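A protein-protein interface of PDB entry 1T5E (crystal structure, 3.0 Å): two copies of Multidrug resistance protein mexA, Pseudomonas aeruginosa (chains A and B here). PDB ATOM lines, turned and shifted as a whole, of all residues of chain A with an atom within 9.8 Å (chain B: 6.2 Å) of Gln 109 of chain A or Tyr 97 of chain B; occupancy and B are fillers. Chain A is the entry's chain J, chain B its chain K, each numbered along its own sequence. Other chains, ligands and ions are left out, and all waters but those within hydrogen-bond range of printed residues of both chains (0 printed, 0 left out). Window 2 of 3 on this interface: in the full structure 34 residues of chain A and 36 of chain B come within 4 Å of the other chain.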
ATOM      1  N   TYR A  97      -2.835   3.495  -4.059  1.00  0.00           N
ATOM      2  CA  TYR A  97      -3.201   2.941  -2.772  1.00  0.00           C
ATOM      3  C   TYR A  97      -2.456   3.619  -1.655  1.00  0.00           C
ATOM      4  O   TYR A  97      -2.932   3.672  -0.525  1.00  0.00           O
ATOM      5  CB  TYR A  97      -2.928   1.458  -2.746  1.00  0.00           C
ATOM      6  CG  TYR A  97      -4.055   0.699  -3.331  1.00  0.00           C
ATOM      7  CD1 TYR A  97      -4.067  -0.684  -3.304  1.00  0.00           C
ATOM      8  CD2 TYR A  97      -5.146   1.364  -3.879  1.00  0.00           C
ATOM      9  CE1 TYR A  97      -5.150  -1.401  -3.804  1.00  0.00           C
ATOM     10  CE2 TYR A  97      -6.231   0.666  -4.383  1.00  0.00           C
ATOM     11  CZ  TYR A  97      -6.226  -0.717  -4.339  1.00  0.00           C
ATOM     12  OH  TYR A  97      -7.298  -1.427  -4.804  1.00  0.00           O
ATOM     13  N   VAL A 101      -4.820   4.295   1.613  1.00  0.00           N
ATOM     14  CA  VAL A 101      -4.622   3.659   2.917  1.00  0.00           C
ATOM     15  C   VAL A 101      -4.473   4.817   3.908  1.00  0.00           C
ATOM     16  O   VAL A 101      -4.835   4.711   5.089  1.00  0.00           O
ATOM     17  CB  VAL A 101      -3.331   2.781   2.937  1.00  0.00           C
ATOM     18  CG1 VAL A 101      -2.092   3.668   2.908  1.00  0.00           C
ATOM     19  CG2 VAL A 101      -3.333   1.860   4.160  1.00  0.00           C
ATOM     20  N   GLN A 104      -7.847   5.676   5.249  1.00  0.00           N
ATOM     21  CA  GLN A 104      -8.678   4.533   5.653  1.00  0.00           C
ATOM     22  C   GLN A 104      -9.549   4.009   4.497  1.00  0.00           C
ATOM     23  O   GLN A 104     -10.366   3.095   4.680  1.00  0.00           O
ATOM     24  CB  GLN A 104      -9.585   4.944   6.824  1.00  0.00           C
ATOM     25  CG  GLN A 104     -10.236   3.790   7.591  1.00  0.00           C
ATOM     26  CD  GLN A 104      -9.342   3.250   8.701  1.00  0.00           C
ATOM     27  OE1 GLN A 104      -9.193   3.874   9.758  1.00  0.00           O
ATOM     28  NE2 GLN A 104      -8.734   2.089   8.460  1.00  0.00           N
ATOM     29  N   ALA A 105      -9.367   4.607   3.317  1.00  0.00           N
ATOM     30  CA  ALA A 105     -10.103   4.236   2.106  1.00  0.00           C
ATOM     31  C   ALA A 105      -9.735   2.828   1.650  1.00  0.00           C
ATOM     32  O   ALA A 105     -10.445   2.216   0.856  1.00  0.00           O
ATOM     33  CB  ALA A 105      -9.799   5.229   0.998  1.00  0.00           C
ATOM     34  N   VAL A 106      -8.616   2.328   2.163  1.00  0.00           N
ATOM     35  CA  VAL A 106      -8.104   1.001   1.840  1.00  0.00           C
ATOM     36  C   VAL A 106      -7.330   0.453   3.050  1.00  0.00           C
ATOM     37  O   VAL A 106      -6.597   1.191   3.726  1.00  0.00           O
ATOM     38  CB  VAL A 106      -7.188   1.078   0.587  1.00  0.00           C
ATOM     39  CG1 VAL A 106      -6.065   0.054   0.661  1.00  0.00           C
ATOM     40  CG2 VAL A 106      -8.022   0.837  -0.653  1.00  0.00           C
ATOM     41  N   SER A 107      -7.501  -0.836   3.327  1.00  0.00           N
ATOM     42  CA  SER A 107      -6.827  -1.457   4.461  1.00  0.00           C
ATOM     43  C   SER A 107      -5.329  -1.527   4.247  1.00  0.00           C
ATOM     44  O   SER A 107      -4.848  -1.391   3.126  1.00  0.00           O
ATOM     45  CB  SER A 107      -7.358  -2.867   4.679  1.00  0.00           C
ATOM     46  OG  SER A 107      -6.940  -3.726   3.634  1.00  0.00           O
ATOM     47  N   LYS A 108      -4.589  -1.745   5.328  1.00  0.00           N
ATOM     48  CA  LYS A 108      -3.143  -1.849   5.227  1.00  0.00           C
ATOM     49  C   LYS A 108      -2.839  -3.134   4.485  1.00  0.00           C
ATOM     50  O   LYS A 108      -1.775  -3.279   3.896  1.00  0.00           O
ATOM     51  CB  LYS A 108      -2.494  -1.910   6.606  1.00  0.00           C
ATOM     52  CG  LYS A 108      -2.608  -0.658   7.460  1.00  0.00           C
ATOM     53  CD  LYS A 108      -1.671  -0.808   8.656  1.00  0.00           C
ATOM     54  CE  LYS A 108      -1.698   0.377   9.612  1.00  0.00           C
ATOM     55  NZ  LYS A 108      -0.669   0.231  10.697  1.00  0.00           N
ATOM     56  N   GLN A 109      -3.783  -4.072   4.533  1.00  0.00           N
ATOM     57  CA  GLN A 109      -3.623  -5.352   3.848  1.00  0.00           C
ATOM     58  C   GLN A 109      -3.622  -5.084   2.346  1.00  0.00           C
ATOM     59  O   GLN A 109      -2.669  -5.444   1.641  1.00  0.00           O
ATOM     60  CB  GLN A 109      -4.767  -6.312   4.211  1.00  0.00           C
ATOM     61  CG  GLN A 109      -4.582  -7.751   3.681  1.00  0.00           C
ATOM     62  CD  GLN A 109      -3.205  -8.328   4.004  1.00  0.00           C
ATOM     63  OE1 GLN A 109      -2.763  -8.316   5.153  1.00  0.00           O
ATOM     64  NE2 GLN A 109      -2.523  -8.842   2.983  1.00  0.00           N
ATOM     65  N   GLN A 110      -4.693  -4.446   1.869  1.00  0.00           N
ATOM     66  CA  GLN A 110      -4.828  -4.087   0.461  1.00  0.00           C
ATOM     67  C   GLN A 110      -3.596  -3.328  -0.016  1.00  0.00           C
ATOM     68  O   GLN A 110      -3.031  -3.648  -1.062  1.00  0.00           O
ATOM     69  CB  GLN A 110      -6.050  -3.210   0.252  1.00  0.00           C
ATOM     70  CG  GLN A 110      -7.361  -3.924   0.443  1.00  0.00           C
ATOM     71  CD  GLN A 110      -8.532  -2.992   0.261  1.00  0.00           C
ATOM     72  OE1 GLN A 110      -8.742  -2.073   1.066  1.00  0.00           O
ATOM     73  NE2 GLN A 110      -9.301  -3.206  -0.808  1.00  0.00           N
ATOM     74  N   TYR A 111      -3.182  -2.319   0.747  1.00  0.00           N
ATOM     75  CA  TYR A 111      -2.013  -1.567   0.363  1.00  0.00           C
ATOM     76  C   TYR A 111      -0.777  -2.447   0.356  1.00  0.00           C
ATOM     77  O   TYR A 111      -0.024  -2.481  -0.609  1.00  0.00           O
ATOM     78  CB  TYR A 111      -1.763  -0.408   1.311  1.00  0.00           C
ATOM     79  CG  TYR A 111      -0.470   0.278   0.976  1.00  0.00           C
ATOM     80  CD1 TYR A 111      -0.425   1.295   0.041  1.00  0.00           C
ATOM     81  CD2 TYR A 111       0.731  -0.206   1.473  1.00  0.00           C
ATOM     82  CE1 TYR A 111       0.788   1.804  -0.408  1.00  0.00           C
ATOM     83  CE2 TYR A 111       1.945   0.288   1.038  1.00  0.00           C
ATOM     84  CZ  TYR A 111       1.976   1.291   0.094  1.00  0.00           C
ATOM     85  OH  TYR A 111       3.193   1.746  -0.363  1.00  0.00           O
ATOM     86  N   ALA A 112      -0.545  -3.135   1.464  1.00  0.00           N
ATOM     87  CA  ALA A 112       0.621  -4.003   1.593  1.00  0.00           C
ATOM     88  C   ALA A 112       0.747  -4.890   0.369  1.00  0.00           C
ATOM     89  O   ALA A 112       1.797  -4.932  -0.283  1.00  0.00           O
ATOM     90  CB  ALA A 112       0.498  -4.863   2.856  1.00  0.00           C
ATOM     91  N   ASP A 113      -0.337  -5.593   0.058  1.00  0.00           N
ATOM     92  CA  ASP A 113      -0.353  -6.495  -1.086  1.00  0.00           C
ATOM     93  C   ASP A 113      -0.012  -5.758  -2.370  1.00  0.00           C
ATOM     94  O   ASP A 113       0.734  -6.266  -3.207  1.00  0.00           O
ATOM     95  CB  ASP A 113      -1.725  -7.151  -1.252  1.00  0.00           C
ATOM     96  CG  ASP A 113      -2.115  -8.028  -0.074  1.00  0.00           C
ATOM     97  OD1 ASP A 113      -1.308  -8.901   0.332  1.00  0.00           O
ATOM     98  OD2 ASP A 113      -3.249  -7.848   0.433  1.00  0.00           O
ATOM     99  N   ALA A 114      -0.581  -4.563  -2.521  1.00  0.00           N
ATOM    100  CA  ALA A 114      -0.347  -3.732  -3.697  1.00  0.00           C
ATOM    101  C   ALA A 114       1.131  -3.401  -3.842  1.00  0.00           C
ATOM    102  O   ALA A 114       1.695  -3.544  -4.919  1.00  0.00           O
ATOM    103  CB  ALA A 114      -1.158  -2.449  -3.603  1.00  0.00           C
ATOM    104  N   ASN A 115       1.767  -2.971  -2.762  1.00  0.00           N
ATOM    105  CA  ASN A 115       3.168  -2.630  -2.849  1.00  0.00           C
ATOM    106  C   ASN A 115       3.991  -3.887  -3.048  1.00  0.00           C
ATOM    107  O   ASN A 115       5.122  -3.849  -3.542  1.00  0.00           O
ATOM    108  CB  ASN A 115       3.603  -1.897  -1.587  1.00  0.00           C
ATOM    109  CG  ASN A 115       4.948  -1.239  -1.741  1.00  0.00           C
ATOM    110  OD1 ASN A 115       5.972  -1.898  -1.643  1.00  0.00           O
ATOM    111  ND2 ASN A 115       4.954   0.069  -2.003  1.00  0.00           N
ATOM    112  N   ALA A 116       3.407  -5.014  -2.660  1.00  0.00           N
ATOM    113  CA  ALA A 116       4.081  -6.301  -2.788  1.00  0.00           C
ATOM    114  C   ALA A 116       4.199  -6.620  -4.271  1.00  0.00           C
ATOM    115  O   ALA A 116       5.282  -6.931  -4.775  1.00  0.00           O
ATOM    116  CB  ALA A 116       3.282  -7.378  -2.087  1.00  0.00           C
ATOM    117  N   ALA A 117       3.070  -6.523  -4.965  1.00  0.00           N
ATOM    118  CA  ALA A 117       3.024  -6.791  -6.393  1.00  0.00           C
ATOM    119  C   ALA A 117       3.964  -5.839  -7.111  1.00  0.00           C
ATOM    120  O   ALA A 117       4.739  -6.258  -7.976  1.00  0.00           O
ATOM    121  CB  ALA A 117       1.615  -6.629  -6.909  1.00  0.00           C
ATOM    122  N   GLU B  92       7.140  -6.783   6.860  1.00  0.00           N
ATOM    123  CA  GLU B  92       6.072  -5.884   7.265  1.00  0.00           C
ATOM    124  C   GLU B  92       4.863  -6.760   7.583  1.00  0.00           C
ATOM    125  O   GLU B  92       4.289  -6.653   8.662  1.00  0.00           O
ATOM    126  CB  GLU B  92       5.762  -4.893   6.131  1.00  0.00           C
ATOM    127  CG  GLU B  92       4.722  -3.840   6.458  1.00  0.00           C
ATOM    128  CD  GLU B  92       3.318  -4.411   6.511  1.00  0.00           C
ATOM    129  OE1 GLU B  92       2.964  -5.182   5.583  1.00  0.00           O
ATOM    130  OE2 GLU B  92       2.568  -4.088   7.465  1.00  0.00           O
ATOM    131  N   GLN B  93       4.501  -7.635   6.646  1.00  0.00           N
ATOM    132  CA  GLN B  93       3.364  -8.537   6.814  1.00  0.00           C
ATOM    133  C   GLN B  93       3.362  -9.161   8.211  1.00  0.00           C
ATOM    134  O   GLN B  93       2.368  -9.099   8.945  1.00  0.00           O
ATOM    135  CB  GLN B  93       3.435  -9.649   5.770  1.00  0.00           C
ATOM    136  CG  GLN B  93       2.317 -10.656   5.849  1.00  0.00           C
ATOM    137  CD  GLN B  93       1.054 -10.133   5.235  1.00  0.00           C
ATOM    138  OE1 GLN B  93       0.595  -9.050   5.575  1.00  0.00           O
ATOM    139  NE2 GLN B  93       0.478 -10.895   4.318  1.00  0.00           N
ATOM    140  N   ALA B  94       4.495  -9.768   8.561  1.00  0.00           N
ATOM    141  CA  ALA B  94       4.680 -10.417   9.849  1.00  0.00           C
ATOM    142  C   ALA B  94       4.427  -9.430  10.981  1.00  0.00           C
ATOM    143  O   ALA B  94       3.419  -9.530  11.679  1.00  0.00           O
ATOM    144  CB  ALA B  94       6.088 -10.979   9.944  1.00  0.00           C
ATOM    145  N   GLN B  95       5.334  -8.472  11.156  1.00  0.00           N
ATOM    146  CA  GLN B  95       5.202  -7.464  12.208  1.00  0.00           C
ATOM    147  C   GLN B  95       3.765  -6.982  12.409  1.00  0.00           C
ATOM    148  O   GLN B  95       3.357  -6.650  13.523  1.00  0.00           O
ATOM    149  CB  GLN B  95       6.085  -6.258  11.896  1.00  0.00           C
ATOM    150  CG  GLN B  95       7.561  -6.569  11.905  1.00  0.00           C
ATOM    151  CD  GLN B  95       8.408  -5.411  11.415  1.00  0.00           C
ATOM    152  OE1 GLN B  95       8.418  -4.335  12.014  1.00  0.00           O
ATOM    153  NE2 GLN B  95       9.126  -5.627  10.311  1.00  0.00           N
ATOM    154  N   ARG B  96       2.993  -6.950  11.331  1.00  0.00           N
ATOM    155  CA  ARG B  96       1.625  -6.482  11.428  1.00  0.00           C
ATOM    156  C   ARG B  96       0.707  -7.560  11.986  1.00  0.00           C
ATOM    157  O   ARG B  96       0.003  -7.322  12.972  1.00  0.00           O
ATOM    158  CB  ARG B  96       1.127  -6.004  10.054  1.00  0.00           C
ATOM    159  CG  ARG B  96      -0.054  -5.027  10.122  1.00  0.00           C
ATOM    160  CD  ARG B  96      -0.488  -4.560   8.743  1.00  0.00           C
ATOM    161  NE  ARG B  96      -0.988  -5.657   7.918  1.00  0.00           N
ATOM    162  CZ  ARG B  96      -0.536  -5.929   6.700  1.00  0.00           C
ATOM    163  NH1 ARG B  96       0.424  -5.187   6.175  1.00  0.00           N
ATOM    164  NH2 ARG B  96      -1.042  -6.934   6.006  1.00  0.00           N
ATOM    165  N   TYR B  97       0.705  -8.736  11.358  1.00  0.00           N
ATOM    166  CA  TYR B  97      -0.138  -9.846  11.810  1.00  0.00           C
ATOM    167  C   TYR B  97       0.073 -10.147  13.286  1.00  0.00           C
ATOM    168  O   TYR B  97      -0.849 -10.591  13.970  1.00  0.00           O
ATOM    169  CB  TYR B  97       0.152 -11.101  11.004  1.00  0.00           C
ATOM    170  CG  TYR B  97      -0.673 -11.244   9.763  1.00  0.00           C
ATOM    171  CD1 TYR B  97      -1.074 -10.130   9.034  1.00  0.00           C
ATOM    172  CD2 TYR B  97      -0.987 -12.510   9.263  1.00  0.00           C
ATOM    173  CE1 TYR B  97      -1.770 -10.272   7.815  1.00  0.00           C
ATOM    174  CE2 TYR B  97      -1.678 -12.673   8.053  1.00  0.00           C
ATOM    175  CZ  TYR B  97      -2.066 -11.550   7.327  1.00  0.00           C
ATOM    176  OH  TYR B  97      -2.719 -11.705   6.114  1.00  0.00           O
ATOM    177  N   LYS B  98       1.288  -9.907  13.767  1.00  0.00           N
ATOM    178  CA  LYS B  98       1.621 -10.139  15.163  1.00  0.00           C
ATOM    179  C   LYS B  98       0.632  -9.407  16.086  1.00  0.00           C
ATOM    180  O   LYS B  98      -0.050 -10.024  16.916  1.00  0.00           O
ATOM    181  CB  LYS B  98       3.045  -9.656  15.444  1.00  0.00           C
ATOM    182  CG  LYS B  98       3.777 -10.493  16.477  1.00  0.00           C
ATOM    183  CD  LYS B  98       5.017  -9.805  17.013  1.00  0.00           C
ATOM    184  CE  LYS B  98       5.795 -10.750  17.917  1.00  0.00           C
ATOM    185  NZ  LYS B  98       6.948 -10.085  18.590  1.00  0.00           N
ATOM    186  N   LEU B  99       0.563  -8.087  15.930  1.00  0.00           N
ATOM    187  CA  LEU B  99      -0.324  -7.235  16.721  1.00  0.00           C
ATOM    188  C   LEU B  99      -1.799  -7.500  16.416  1.00  0.00           C
ATOM    189  O   LEU B  99      -2.683  -6.942  17.057  1.00  0.00           O
ATOM    190  CB  LEU B  99      -0.009  -5.757  16.450  1.00  0.00           C
ATOM    191  CG  LEU B  99       1.367  -5.215  16.863  1.00  0.00           C
ATOM    192  CD1 LEU B  99       2.468  -6.124  16.347  1.00  0.00           C
ATOM    193  CD2 LEU B  99       1.545  -3.800  16.330  1.00  0.00           C
ATOM    194  N   LEU B 100      -2.065  -8.361  15.444  1.00  0.00           N
ATOM    195  CA  LEU B 100      -3.442  -8.657  15.073  1.00  0.00           C
ATOM    196  C   LEU B 100      -3.902 -10.016  15.564  1.00  0.00           C
ATOM    197  O   LEU B 100      -5.104 -10.295  15.631  1.00  0.00           O
ATOM    198  CB  LEU B 100      -3.593  -8.555  13.561  1.00  0.00           C
ATOM    199  CG  LEU B 100      -3.206  -7.162  13.078  1.00  0.00           C
ATOM    200  CD1 LEU B 100      -3.349  -7.110  11.581  1.00  0.00           C
ATOM    201  CD2 LEU B 100      -4.080  -6.115  13.759  1.00  0.00           C
ATOM    202  N   VAL B 101      -2.938 -10.867  15.892  1.00  0.00           N
ATOM    203  CA  VAL B 101      -3.239 -12.186  16.423  1.00  0.00           C
ATOM    204  C   VAL B 101      -3.383 -11.908  17.916  1.00  0.00           C
ATOM    205  O   VAL B 101      -4.033 -12.654  18.645  1.00  0.00           O
ATOM    206  CB  VAL B 101      -2.077 -13.178  16.166  1.00  0.00           C
ATOM    207  CG1 VAL B 101      -0.945 -12.918  17.151  1.00  0.00           C
ATOM    208  CG2 VAL B 101      -2.590 -14.617  16.226  1.00  0.00           C
ATOM    209  N   ALA B 102      -2.773 -10.805  18.352  1.00  0.00           N
ATOM    210  CA  ALA B 102      -2.832 -10.373  19.747  1.00  0.00           C
ATOM    211  C   ALA B 102      -4.193  -9.723  20.036  1.00  0.00           C
ATOM    212  O   ALA B 102      -4.356  -9.006  21.027  1.00  0.00           O
ATOM    213  CB  ALA B 102      -1.700  -9.381  20.040  1.00  0.00           C
ATOM    214  N   VAL B 106      -7.108 -12.345  13.973  1.00  0.00           N
ATOM    215  CA  VAL B 106      -6.485 -13.159  12.928  1.00  0.00           C
ATOM    216  C   VAL B 106      -6.249 -14.581  13.443  1.00  0.00           C
ATOM    217  O   VAL B 106      -5.844 -14.777  14.599  1.00  0.00           O
ATOM    218  CB  VAL B 106      -5.113 -12.598  12.503  1.00  0.00           C
ATOM    219  CG1 VAL B 106      -4.651 -13.305  11.241  1.00  0.00           C
ATOM    220  CG2 VAL B 106      -5.186 -11.095  12.302  1.00  0.00           C
ATOM    221  N   GLN B 110      -2.627 -18.543  10.755  1.00  0.00           N
ATOM    222  CA  GLN B 110      -2.193 -17.530   9.811  1.00  0.00           C
ATOM    223  C   GLN B 110      -0.928 -16.806  10.254  1.00  0.00           C
ATOM    224  O   GLN B 110       0.062 -16.808   9.525  1.00  0.00           O
ATOM    225  CB  GLN B 110      -3.314 -16.529   9.589  1.00  0.00           C
ATOM    226  CG  GLN B 110      -4.630 -17.199   9.259  1.00  0.00           C
ATOM    227  CD  GLN B 110      -5.696 -16.207   8.834  1.00  0.00           C
ATOM    228  OE1 GLN B 110      -5.777 -15.087   9.365  1.00  0.00           O
ATOM    229  NE2 GLN B 110      -6.536 -16.616   7.879  1.00  0.00           N
ATOM    230  N   TYR B 111      -0.946 -16.190  11.434  1.00  0.00           N
ATOM    231  CA  TYR B 111       0.240 -15.485  11.897  1.00  0.00           C
ATOM    232  C   TYR B 111       1.482 -16.354  11.815  1.00  0.00           C
ATOM    233  O   TYR B 111       2.587 -15.861  11.597  1.00  0.00           O
ATOM    234  CB  TYR B 111       0.115 -15.026  13.335  1.00  0.00           C
ATOM    235  CG  TYR B 111       1.447 -14.529  13.828  1.00  0.00           C
ATOM    236  CD1 TYR B 111       1.822 -13.204  13.662  1.00  0.00           C
ATOM    237  CD2 TYR B 111       2.382 -15.408  14.360  1.00  0.00           C
ATOM    238  CE1 TYR B 111       3.093 -12.769  14.011  1.00  0.00           C
ATOM    239  CE2 TYR B 111       3.656 -14.983  14.705  1.00  0.00           C
ATOM    240  CZ  TYR B 111       4.005 -13.665  14.533  1.00  0.00           C
ATOM    241  OH  TYR B 111       5.255 -13.232  14.916  1.00  0.00           O
ATOM    242  N   ALA B 114       2.686 -16.346   8.309  1.00  0.00           N
ATOM    243  CA  ALA B 114       3.279 -15.056   8.025  1.00  0.00           C
ATOM    244  C   ALA B 114       4.708 -15.012   8.535  1.00  0.00           C
ATOM    245  O   ALA B 114       5.608 -14.565   7.829  1.00  0.00           O
ATOM    246  CB  ALA B 114       2.466 -13.947   8.666  1.00  0.00           C
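Ser 107 of chain A touches none of the printed residues of chain B. Of the printed residues of chain B, Lys 108 of chain A touches Arg 96. Of chain B, only Gln 93, Arg 96 and Tyr 97 come within 4 Å of Gln 109 of chain A. Of the printed residues of chain B, Ala 112 of chain A touches Glu 92 (3.7 Å) and Arg 96 (3.3 Å). Printed residues of chain A within 4 Å of Glu 92 of chain B: Ala 112 (3.7 Å). Printed residues of chain A within 4 Å of Gln 93 of chain B: Gln 109 (3.5 Å). Arg 96 of chain B touches just these residues of chain A: Lys 108, Gln 109 and Ala 112. Tyr 97 of chain B touches one residue of chain A. Ala 114 of chain B touches none of the printed residues of chain A. The nearest printed residue of chain B that does not touch Gln 109 of chain A is Glu 92 of chain B (6.5 Å).
Among the printed residues, merely in contact across the chains: Lys 108 of chain A with Arg 96 of chain B (3.7 Å), Gln 109 of chain A with Tyr 97 of chain B (3.4 Å), Ala 112 of chain A with Glu 92 of chain B (3.7 Å) and Ala 112 of chain A with Arg 96 of chain B (3.3 Å).
Of the 15 printed residues of chain B, 4 touch a printed residue of chain A. Printed residues of chain B that touch a printed residue of chain A: Glu 92, Gln 93, Arg 96 and Tyr 97. Hydrophobic or aromatic side chains of chain B within 4 Å of the printed part of chain A: Tyr 97. Among the printed residues, 6 pairs touch across the chains.
Positions printed for both chains: 97, 101, 106, 110, 111 and 114.
The side-chain amide oxygen (OE1) of Gln 109 of chain A sits close to the side-chain amide oxygen (OE1) of Gln 93 of chain B. The side-chain amide oxygen (OE1) of Gln 109 of chain A sits close to the guanidinium group (NH2) of Arg 96 of chain B (2.4 Å).
The side-chain amide oxygen of Gln 93 of chain B sits at hydrogen-bond distance from the guanidinium group of Arg 96 of chain B (2.7 Å). OG of Ser 107 of chain A sits close to N of Gln 109 of chain A (3.3 Å). The side-chain amide nitrogen (NE2) of Gln 109 of chain A is in hydrogen-bond range of the side-chain carboxylate (OD2) of Asp 113 of chain A. OE1 of Glu 92 of chain B lies within salt-bridge range of NH1 of Arg 96 of chain B (2.6 Å).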
